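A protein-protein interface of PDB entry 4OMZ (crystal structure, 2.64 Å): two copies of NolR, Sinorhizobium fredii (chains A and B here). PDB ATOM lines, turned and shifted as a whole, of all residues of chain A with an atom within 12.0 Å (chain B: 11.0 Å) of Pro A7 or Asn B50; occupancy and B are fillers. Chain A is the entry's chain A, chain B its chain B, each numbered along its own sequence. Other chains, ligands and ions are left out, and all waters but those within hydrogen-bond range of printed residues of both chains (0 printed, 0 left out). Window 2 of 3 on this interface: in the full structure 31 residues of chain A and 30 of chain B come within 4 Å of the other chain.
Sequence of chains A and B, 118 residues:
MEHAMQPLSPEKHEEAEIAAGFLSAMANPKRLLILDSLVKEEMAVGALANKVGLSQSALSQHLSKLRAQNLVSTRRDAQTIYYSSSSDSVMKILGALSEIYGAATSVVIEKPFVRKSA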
ATOM      1  N   GLN A   6       4.280   8.295  13.017  1.00  0.00           N
ATOM      2  CA  GLN A   6       4.539   7.316  14.066  1.00  0.00           C
ATOM      3  C   GLN A   6       3.329   6.395  14.300  1.00  0.00           C
ATOM      4  O   GLN A   6       2.271   6.842  14.757  1.00  0.00           O
ATOM      5  CB  GLN A   6       4.925   8.041  15.361  1.00  0.00           C
ATOM      6  CG  GLN A   6       3.935   9.135  15.763  1.00  0.00           C
ATOM      7  CD  GLN A   6       4.306   9.845  17.050  1.00  0.00           C
ATOM      8  OE1 GLN A   6       5.475   9.901  17.438  1.00  0.00           O
ATOM      9  NE2 GLN A   6       3.297  10.369  17.739  1.00  0.00           N
ATOM     10  N   PRO A   7       3.470   5.104  13.949  1.00  0.00           N
ATOM     11  CA  PRO A   7       2.437   4.092  14.219  1.00  0.00           C
ATOM     12  C   PRO A   7       2.123   3.894  15.706  1.00  0.00           C
ATOM     13  O   PRO A   7       2.872   4.350  16.572  1.00  0.00           O
ATOM     14  CB  PRO A   7       3.037   2.816  13.619  1.00  0.00           C
ATOM     15  CG  PRO A   7       3.993   3.298  12.586  1.00  0.00           C
ATOM     16  CD  PRO A   7       4.579   4.555  13.151  1.00  0.00           C
ATOM     17  N   LEU A   8       1.005   3.228  15.982  1.00  0.00           N
ATOM     18  CA  LEU A   8       0.576   2.950  17.351  1.00  0.00           C
ATOM     19  C   LEU A   8       1.380   1.795  17.951  1.00  0.00           C
ATOM     20  O   LEU A   8       1.724   0.848  17.245  1.00  0.00           O
ATOM     21  CB  LEU A   8      -0.923   2.637  17.393  1.00  0.00           C
ATOM     22  CG  LEU A   8      -1.854   3.823  17.120  1.00  0.00           C
ATOM     23  CD1 LEU A   8      -3.271   3.353  16.838  1.00  0.00           C
ATOM     24  CD2 LEU A   8      -1.833   4.806  18.282  1.00  0.00           C
ATOM     25  N   SER A   9       1.698   1.881  19.239  1.00  0.00           N
ATOM     26  CA  SER A   9       2.461   0.828  19.910  1.00  0.00           C
ATOM     27  C   SER A   9       1.745  -0.523  19.831  1.00  0.00           C
ATOM     28  O   SER A   9       0.518  -0.574  19.704  1.00  0.00           O
ATOM     29  CB  SER A   9       2.716   1.198  21.373  1.00  0.00           C
ATOM     30  OG  SER A   9       1.595   0.876  22.180  1.00  0.00           O
ATOM     31  N   PRO A  10       2.511  -1.625  19.907  1.00  0.00           N
ATOM     32  CA  PRO A  10       1.931  -2.971  19.942  1.00  0.00           C
ATOM     33  C   PRO A  10       0.998  -3.168  21.138  1.00  0.00           C
ATOM     34  O   PRO A  10       0.048  -3.958  21.058  1.00  0.00           O
ATOM     35  CB  PRO A  10       3.161  -3.875  20.034  1.00  0.00           C
ATOM     36  CG  PRO A  10       4.229  -3.088  19.352  1.00  0.00           C
ATOM     37  CD  PRO A  10       3.979  -1.674  19.787  1.00  0.00           C
ATOM     38  N   GLU A  11       1.262  -2.457  22.231  1.00  0.00           N
ATOM     39  CA  GLU A  11       0.412  -2.555  23.412  1.00  0.00           C
ATOM     40  C   GLU A  11      -1.023  -2.111  23.146  1.00  0.00           C
ATOM     41  O   GLU A  11      -1.961  -2.761  23.594  1.00  0.00           O
ATOM     42  CB  GLU A  11       0.981  -1.714  24.561  1.00  0.00           C
ATOM     43  CG  GLU A  11       0.281  -1.954  25.897  1.00  0.00           C
ATOM     44  CD  GLU A  11       0.988  -1.306  27.079  1.00  0.00           C
ATOM     45  OE1 GLU A  11       1.922  -0.504  26.859  1.00  0.00           O
ATOM     46  OE2 GLU A  11       0.596  -1.591  28.233  1.00  0.00           O
ATOM     47  N   LYS A  12      -1.191  -1.014  22.410  1.00  0.00           N
ATOM     48  CA  LYS A  12      -2.522  -0.478  22.095  1.00  0.00           C
ATOM     49  C   LYS A  12      -3.268  -1.340  21.081  1.00  0.00           C
ATOM     50  O   LYS A  12      -4.494  -1.363  21.017  1.00  0.00           O
ATOM     51  CB  LYS A  12      -2.392   0.966  21.627  1.00  0.00           C
ATOM     52  CG  LYS A  12      -1.802   1.830  22.729  1.00  0.00           C
ATOM     53  CD  LYS A  12      -1.685   3.309  22.371  1.00  0.00           C
ATOM     54  CE  LYS A  12      -2.779   4.110  23.082  1.00  0.00           C
ATOM     55  NZ  LYS A  12      -3.141   5.388  22.394  1.00  0.00           N
ATOM     56  N   HIS A  13      -2.472  -2.037  20.295  1.00  0.00           N
ATOM     57  CA  HIS A  13      -2.876  -3.035  19.320  1.00  0.00           C
ATOM     58  C   HIS A  13      -3.465  -4.280  20.000  1.00  0.00           C
ATOM     59  O   HIS A  13      -4.547  -4.799  19.625  1.00  0.00           O
ATOM     60  CB  HIS A  13      -1.598  -3.298  18.519  1.00  0.00           C
ATOM     61  CG  HIS A  13      -1.545  -2.570  17.214  1.00  0.00           C
ATOM     62  ND1 HIS A  13      -2.595  -1.814  16.767  1.00  0.00           N
ATOM     63  CD2 HIS A  13      -0.493  -2.240  16.426  1.00  0.00           C
ATOM     64  CE1 HIS A  13      -2.263  -1.229  15.632  1.00  0.00           C
ATOM     65  NE2 HIS A  13      -0.977  -1.429  15.433  1.00  0.00           N
ATOM     66  N   GLU A  14      -2.800  -4.679  21.075  1.00  0.00           N
ATOM     67  CA  GLU A  14      -3.211  -5.824  21.864  1.00  0.00           C
ATOM     68  C   GLU A  14      -4.415  -5.480  22.762  1.00  0.00           C
ATOM     69  O   GLU A  14      -5.333  -6.297  22.974  1.00  0.00           O
ATOM     70  CB  GLU A  14      -2.023  -6.256  22.721  1.00  0.00           C
ATOM     71  CG  GLU A  14      -1.011  -7.139  22.015  1.00  0.00           C
ATOM     72  CD  GLU A  14       0.097  -7.589  22.945  1.00  0.00           C
ATOM     73  OE1 GLU A  14       0.159  -7.076  24.086  1.00  0.00           O
ATOM     74  OE2 GLU A  14       0.909  -8.444  22.537  1.00  0.00           O
ATOM     75  N   ALA A  16      -6.613  -3.101  21.965  1.00  0.00           N
ATOM     76  CA  ALA A  16      -7.710  -2.980  21.023  1.00  0.00           C
ATOM     77  C   ALA A  16      -8.265  -4.368  20.746  1.00  0.00           C
ATOM     78  O   ALA A  16      -9.476  -4.537  20.586  1.00  0.00           O
ATOM     79  CB  ALA A  16      -7.250  -2.315  19.747  1.00  0.00           C
ATOM     80  N   LYS B  30      -9.302  -2.824  14.819  1.00  0.00           N
ATOM     81  CA  LYS B  30      -8.815  -1.811  13.896  1.00  0.00           C
ATOM     82  C   LYS B  30      -9.710  -0.587  13.965  1.00  0.00           C
ATOM     83  O   LYS B  30      -9.233   0.538  13.997  1.00  0.00           O
ATOM     84  CB  LYS B  30      -8.762  -2.348  12.468  1.00  0.00           C
ATOM     85  CG  LYS B  30      -7.363  -2.472  11.918  1.00  0.00           C
ATOM     86  CD  LYS B  30      -6.559  -3.514  12.667  1.00  0.00           C
ATOM     87  CE  LYS B  30      -5.077  -3.373  12.368  1.00  0.00           C
ATOM     88  NZ  LYS B  30      -4.319  -4.550  12.865  1.00  0.00           N
ATOM     89  N   LEU B  33      -8.986   1.383  17.045  1.00  0.00           N
ATOM     90  CA  LEU B  33      -7.791   2.215  16.896  1.00  0.00           C
ATOM     91  C   LEU B  33      -8.062   3.436  16.020  1.00  0.00           C
ATOM     92  O   LEU B  33      -7.647   4.558  16.342  1.00  0.00           O
ATOM     93  CB  LEU B  33      -6.663   1.391  16.308  1.00  0.00           C
ATOM     94  CG  LEU B  33      -6.209   0.277  17.237  1.00  0.00           C
ATOM     95  CD1 LEU B  33      -5.320  -0.581  16.438  1.00  0.00           C
ATOM     96  CD2 LEU B  33      -5.457   0.826  18.443  1.00  0.00           C
ATOM     97  N   ILE B  34      -8.776   3.208  14.923  1.00  0.00           N
ATOM     98  CA  ILE B  34      -9.195   4.276  14.029  1.00  0.00           C
ATOM     99  C   ILE B  34     -10.003   5.348  14.751  1.00  0.00           C
ATOM    100  O   ILE B  34      -9.670   6.528  14.683  1.00  0.00           O
ATOM    101  CB  ILE B  34     -10.048   3.730  12.869  1.00  0.00           C
ATOM    102  CG1 ILE B  34      -9.187   2.913  11.908  1.00  0.00           C
ATOM    103  CG2 ILE B  34     -10.729   4.863  12.125  1.00  0.00           C
ATOM    104  CD1 ILE B  34      -9.992   2.017  10.986  1.00  0.00           C
ATOM    105  N   SER B  37      -7.965   7.308  17.292  1.00  0.00           N
ATOM    106  CA  SER B  37      -7.151   8.302  16.593  1.00  0.00           C
ATOM    107  C   SER B  37      -7.961   9.495  16.074  1.00  0.00           C
ATOM    108  O   SER B  37      -7.550  10.645  16.225  1.00  0.00           O
ATOM    109  CB  SER B  37      -6.422   7.645  15.424  1.00  0.00           C
ATOM    110  OG  SER B  37      -5.779   6.457  15.851  1.00  0.00           O
ATOM    111  N   LEU B  38      -9.113   9.214  15.467  1.00  0.00           N
ATOM    112  CA  LEU B  38      -9.951  10.247  14.855  1.00  0.00           C
ATOM    113  C   LEU B  38     -10.639  11.161  15.863  1.00  0.00           C
ATOM    114  O   LEU B  38     -11.018  12.281  15.521  1.00  0.00           O
ATOM    115  CB  LEU B  38     -11.007   9.595  13.961  1.00  0.00           C
ATOM    116  CG  LEU B  38     -10.455   8.952  12.689  1.00  0.00           C
ATOM    117  CD1 LEU B  38     -11.583   8.559  11.754  1.00  0.00           C
ATOM    118  CD2 LEU B  38      -9.504   9.907  12.010  1.00  0.00           C
ATOM    119  N   MET B  43      -7.402  13.595  10.296  1.00  0.00           N
ATOM    120  CA  MET B  43      -6.352  12.836   9.626  1.00  0.00           C
ATOM    121  C   MET B  43      -6.708  12.500   8.190  1.00  0.00           C
ATOM    122  O   MET B  43      -7.835  12.098   7.902  1.00  0.00           O
ATOM    123  CB  MET B  43      -6.052  11.535  10.379  1.00  0.00           C
ATOM    124  CG  MET B  43      -5.437  11.724  11.752  1.00  0.00           C
ATOM    125  SD  MET B  43      -4.814  10.188  12.456  1.00  0.00           S
ATOM    126  CE  MET B  43      -3.107  10.236  11.904  1.00  0.00           C
ATOM    127  N   ALA B  44      -5.730  12.643   7.300  1.00  0.00           N
ATOM    128  CA  ALA B  44      -5.867  12.181   5.926  1.00  0.00           C
ATOM    129  C   ALA B  44      -5.760  10.660   5.875  1.00  0.00           C
ATOM    130  O   ALA B  44      -5.191  10.037   6.776  1.00  0.00           O
ATOM    131  CB  ALA B  44      -4.818  12.821   5.038  1.00  0.00           C
ATOM    132  N   VAL B  45      -6.316  10.070   4.824  1.00  0.00           N
ATOM    133  CA  VAL B  45      -6.405   8.619   4.706  1.00  0.00           C
ATOM    134  C   VAL B  45      -5.033   7.939   4.792  1.00  0.00           C
ATOM    135  O   VAL B  45      -4.890   6.892   5.422  1.00  0.00           O
ATOM    136  CB  VAL B  45      -7.091   8.226   3.379  1.00  0.00           C
ATOM    137  CG1 VAL B  45      -7.147   6.722   3.230  1.00  0.00           C
ATOM    138  CG2 VAL B  45      -8.496   8.808   3.320  1.00  0.00           C
ATOM    139  N   GLY B  46      -4.017   8.551   4.191  1.00  0.00           N
ATOM    140  CA  GLY B  46      -2.675   7.996   4.223  1.00  0.00           C
ATOM    141  C   GLY B  46      -2.090   7.938   5.621  1.00  0.00           C
ATOM    142  O   GLY B  46      -1.654   6.878   6.084  1.00  0.00           O
ATOM    143  N   ALA B  47      -2.082   9.086   6.293  1.00  0.00           N
ATOM    144  CA  ALA B  47      -1.560   9.192   7.651  1.00  0.00           C
ATOM    145  C   ALA B  47      -2.312   8.269   8.610  1.00  0.00           C
ATOM    146  O   ALA B  47      -1.716   7.662   9.498  1.00  0.00           O
ATOM    147  CB  ALA B  47      -1.634  10.636   8.135  1.00  0.00           C
ATOM    148  N   LEU B  48      -3.621   8.159   8.420  1.00  0.00           N
ATOM    149  CA  LEU B  48      -4.434   7.289   9.260  1.00  0.00           C
ATOM    150  C   LEU B  48      -4.061   5.830   9.024  1.00  0.00           C
ATOM    151  O   LEU B  48      -3.957   5.038   9.969  1.00  0.00           O
ATOM    152  CB  LEU B  48      -5.924   7.515   9.002  1.00  0.00           C
ATOM    153  CG  LEU B  48      -6.845   6.659   9.871  1.00  0.00           C
ATOM    154  CD1 LEU B  48      -6.600   6.946  11.341  1.00  0.00           C
ATOM    155  CD2 LEU B  48      -8.297   6.931   9.524  1.00  0.00           C
ATOM    156  N   ALA B  49      -3.907   5.469   7.753  1.00  0.00           N
ATOM    157  CA  ALA B  49      -3.524   4.111   7.395  1.00  0.00           C
ATOM    158  C   ALA B  49      -2.174   3.761   8.011  1.00  0.00           C
ATOM    159  O   ALA B  49      -1.961   2.641   8.476  1.00  0.00           O
ATOM    160  CB  ALA B  49      -3.475   3.951   5.886  1.00  0.00           C
ATOM    161  N   ASN B  50      -1.272   4.735   8.046  1.00  0.00           N
ATOM    162  CA  ASN B  50       0.044   4.512   8.631  1.00  0.00           C
ATOM    163  C   ASN B  50      -0.018   4.389  10.148  1.00  0.00           C
ATOM    164  O   ASN B  50       0.673   3.562  10.745  1.00  0.00           O
ATOM    165  CB  ASN B  50       1.002   5.637   8.246  1.00  0.00           C
ATOM    166  CG  ASN B  50       2.439   5.323   8.611  1.00  0.00           C
ATOM    167  OD1 ASN B  50       2.957   4.266   8.258  1.00  0.00           O
ATOM    168  ND2 ASN B  50       3.089   6.237   9.328  1.00  0.00           N
ATOM    169  N   LYS B  51      -0.865   5.206  10.763  1.00  0.00           N
ATOM    170  CA  LYS B  51      -1.024   5.207  12.211  1.00  0.00           C
ATOM    171  C   LYS B  51      -1.646   3.916  12.730  1.00  0.00           C
ATOM    172  O   LYS B  51      -1.206   3.359  13.739  1.00  0.00           O
ATOM    173  CB  LYS B  51      -1.891   6.401  12.628  1.00  0.00           C
ATOM    174  CG  LYS B  51      -2.232   6.470  14.104  1.00  0.00           C
ATOM    175  CD  LYS B  51      -1.511   7.627  14.784  1.00  0.00           C
ATOM    176  CE  LYS B  51      -1.997   7.819  16.217  1.00  0.00           C
ATOM    177  NZ  LYS B  51      -1.762   9.207  16.695  1.00  0.00           N
ATOM    178  N   VAL B  52      -2.636   3.418  12.002  1.00  0.00           N
ATOM    179  CA  VAL B  52      -3.397   2.253  12.427  1.00  0.00           C
ATOM    180  C   VAL B  52      -2.746   0.975  11.886  1.00  0.00           C
ATOM    181  O   VAL B  52      -3.072  -0.142  12.298  1.00  0.00           O
ATOM    182  CB  VAL B  52      -4.872   2.414  11.967  1.00  0.00           C
ATOM    183  CG1 VAL B  52      -5.663   1.116  12.041  1.00  0.00           C
ATOM    184  CG2 VAL B  52      -5.543   3.497  12.797  1.00  0.00           C
ATOM    185  N   GLY B  53      -1.751   1.154  11.025  1.00  0.00           N
ATOM    186  CA  GLY B  53      -1.060   0.033  10.422  1.00  0.00           C
ATOM    187  C   GLY B  53      -1.981  -0.734   9.496  1.00  0.00           C
ATOM    188  O   GLY B  53      -2.224  -1.927   9.689  1.00  0.00           O
ATOM    189  N   LEU B  54      -2.488  -0.045   8.479  1.00  0.00           N
ATOM    190  CA  LEU B  54      -3.366  -0.663   7.497  1.00  0.00           C
ATOM    191  C   LEU B  54      -3.012  -0.193   6.101  1.00  0.00           C
ATOM    192  O   LEU B  54      -2.392   0.855   5.922  1.00  0.00           O
ATOM    193  CB  LEU B  54      -4.829  -0.303   7.782  1.00  0.00           C
ATOM    194  CG  LEU B  54      -5.617  -0.939   8.925  1.00  0.00           C
ATOM    195  CD1 LEU B  54      -7.055  -0.438   8.882  1.00  0.00           C
ATOM    196  CD2 LEU B  54      -5.576  -2.457   8.820  1.00  0.00           C
ATOM    197  N   SER B  55      -3.425  -0.971   5.108  1.00  0.00           N
ATOM    198  CA  SER B  55      -3.290  -0.569   3.721  1.00  0.00           C
ATOM    199  C   SER B  55      -4.575   0.158   3.355  1.00  0.00           C
ATOM    200  O   SER B  55      -5.542   0.125   4.117  1.00  0.00           O
ATOM    201  CB  SER B  55      -2.996  -1.763   2.810  1.00  0.00           C
ATOM    202  OG  SER B  55      -4.079  -2.665   2.762  1.00  0.00           O
ATOM    203  N   GLN B  56      -4.593   0.825   2.209  1.00  0.00           N
ATOM    204  CA  GLN B  56      -5.720   1.682   1.884  1.00  0.00           C
ATOM    205  C   GLN B  56      -6.998   0.877   1.636  1.00  0.00           C
ATOM    206  O   GLN B  56      -8.103   1.405   1.758  1.00  0.00           O
ATOM    207  CB  GLN B  56      -5.389   2.531   0.655  1.00  0.00           C
ATOM    208  CG  GLN B  56      -4.063   3.277   0.746  1.00  0.00           C
ATOM    209  CD  GLN B  56      -4.121   4.509   1.632  1.00  0.00           C
ATOM    210  OE1 GLN B  56      -4.937   4.592   2.551  1.00  0.00           O
ATOM    211  NE2 GLN B  56      -3.247   5.477   1.360  1.00  0.00           N
ATOM    212  N   SER B  57      -6.843  -0.406   1.323  1.00  0.00           N
ATOM    213  CA  SER B  57      -7.982  -1.297   1.102  1.00  0.00           C
ATOM    214  C   SER B  57      -8.783  -1.542   2.387  1.00  0.00           C
ATOM    215  O   SER B  57      -9.990  -1.262   2.450  1.00  0.00           O
ATOM    216  CB  SER B  57      -7.486  -2.627   0.520  1.00  0.00           C
ATOM    217  OG  SER B  57      -8.534  -3.561   0.363  1.00  0.00           O
ATOM    218  N   ALA B  58      -8.104  -2.045   3.416  1.00  0.00           N
ATOM    219  CA  ALA B  58      -8.747  -2.329   4.688  1.00  0.00           C
ATOM    220  C   ALA B  58      -9.249  -1.046   5.320  1.00  0.00           C
ATOM    221  O   ALA B  58     -10.341  -1.023   5.875  1.00  0.00           O
ATOM    222  CB  ALA B  58      -7.788  -3.057   5.637  1.00  0.00           C
ATOM    223  N   LEU B  59      -8.454   0.019   5.243  1.00  0.00           N
ATOM    224  CA  LEU B  59      -8.867   1.292   5.816  1.00  0.00           C
ATOM    225  C   LEU B  59     -10.120   1.807   5.122  1.00  0.00           C
ATOM    226  O   LEU B  59     -11.021   2.319   5.779  1.00  0.00           O
ATOM    227  CB  LEU B  59      -7.752   2.333   5.732  1.00  0.00           C
ATOM    228  CG  LEU B  59      -8.154   3.695   6.312  1.00  0.00           C
ATOM    229  CD1 LEU B  59      -8.572   3.579   7.772  1.00  0.00           C
ATOM    230  CD2 LEU B  59      -7.022   4.676   6.173  1.00  0.00           C
ATOM    231  N   SER B  60     -10.174   1.672   3.799  1.00  0.00           N
ATOM    232  CA  SER B  60     -11.362   2.069   3.048  1.00  0.00           C
ATOM    233  C   SER B  60     -12.573   1.281   3.542  1.00  0.00           C
ATOM    234  O   SER B  60     -13.635   1.851   3.803  1.00  0.00           O
ATOM    235  CB  SER B  60     -11.159   1.851   1.547  1.00  0.00           C
ATOM    236  OG  SER B  60     -12.362   2.076   0.833  1.00  0.00           O
ATOM    237  N   LEU B  63     -13.529   2.406   7.150  1.00  0.00           N
ATOM    238  CA  LEU B  63     -14.112   3.743   7.101  1.00  0.00           C
ATOM    239  C   LEU B  63     -15.519   3.696   6.541  1.00  0.00           C
ATOM    240  O   LEU B  63     -16.394   4.436   6.982  1.00  0.00           O
ATOM    241  CB  LEU B  63     -13.256   4.696   6.260  1.00  0.00           C
ATOM    242  CG  LEU B  63     -11.961   5.241   6.871  1.00  0.00           C
ATOM    243  CD1 LEU B  63     -11.276   6.197   5.903  1.00  0.00           C
ATOM    244  CD2 LEU B  63     -12.230   5.933   8.202  1.00  0.00           C
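The backbone carbonyl oxygen (O) of Lys B51 is in hydrogen-bond range of the backbone NH (N) of Leu A8 (3.2 Å).
The side-chain hydroxyl (OG) of Ser A9 lies within hydrogen-bond range of the backbone NH (N) of Lys A12 (3.4 Å).
The backbone carbonyl oxygen of Leu B33 is in hydrogen-bond range of the side-chain hydroxyl of Ser B37 (2.7 Å).
Among the printed residues, pairs that only touch across the chains: Gln A6 with Lys B51, Pro A7 with Asn B50, Pro A7 with Lys B51, Leu A8 with Leu B33, Lys A12 with Leu B33, His A13 with Leu B33, His A13 with Val B52 and Ala A16 with Leu B33.
Pro A7 touches just these residues of chain B: Asn B50 and Lys B51.
Of chain B, only Lys B51 (3.9 Å) comes within 4 Å of Gln A6.
Leu A8 touches two residues of chain B.
No residue of chain A comes within 4 Å of Gly B46.
No residue of chain A comes within 4 Å of Ala B47.
Leu B48 touches none of the printed residues of chain A.
Of chain A, only His A13 comes within 4 Å of Val B52.
Printed residues of chain B within 4 Å of Lys A12: Leu B33.
Of the printed residues of chain B, His A13 touches Leu B33 (3.0 Å) and Val B52 (3.6 Å).
Of the printed residues of chain A, Leu B33 touches Leu A8 (3.7 Å), Lys A12 (3.5 Å), His A13 (3.0 Å) and Ala A16 (3.8 Å).
Printed residues of chain B within 4 Å of Ala A16: Leu B33 (3.8 Å).
Leu B59 touches none of the printed residues of chain A.
The nearest residue of chain B that does not touch Pro A7 is Val B52 (5.6 Å).
The nearest printed residue of chain B that does not touch His A13 is Lys B30 (4.8 Å).
Of the 10 printed residues of chain A, 6 touch a printed residue of chain B.
Hydrophobic or aromatic side chains of chain A within 4 Å of the printed part of chain B: Pro A7, Leu A8, His A13 and Ala A16.
Hydrophobic or aromatic side chains of chain B that line the printed part of chain A: Leu B33.
Among the printed residues, 9 pairs touch across the chains.
No position is printed for both chains.
Of the 9 pairs that touch across the chains among the printed residues, none has its exchanged pair printed and touching as well.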
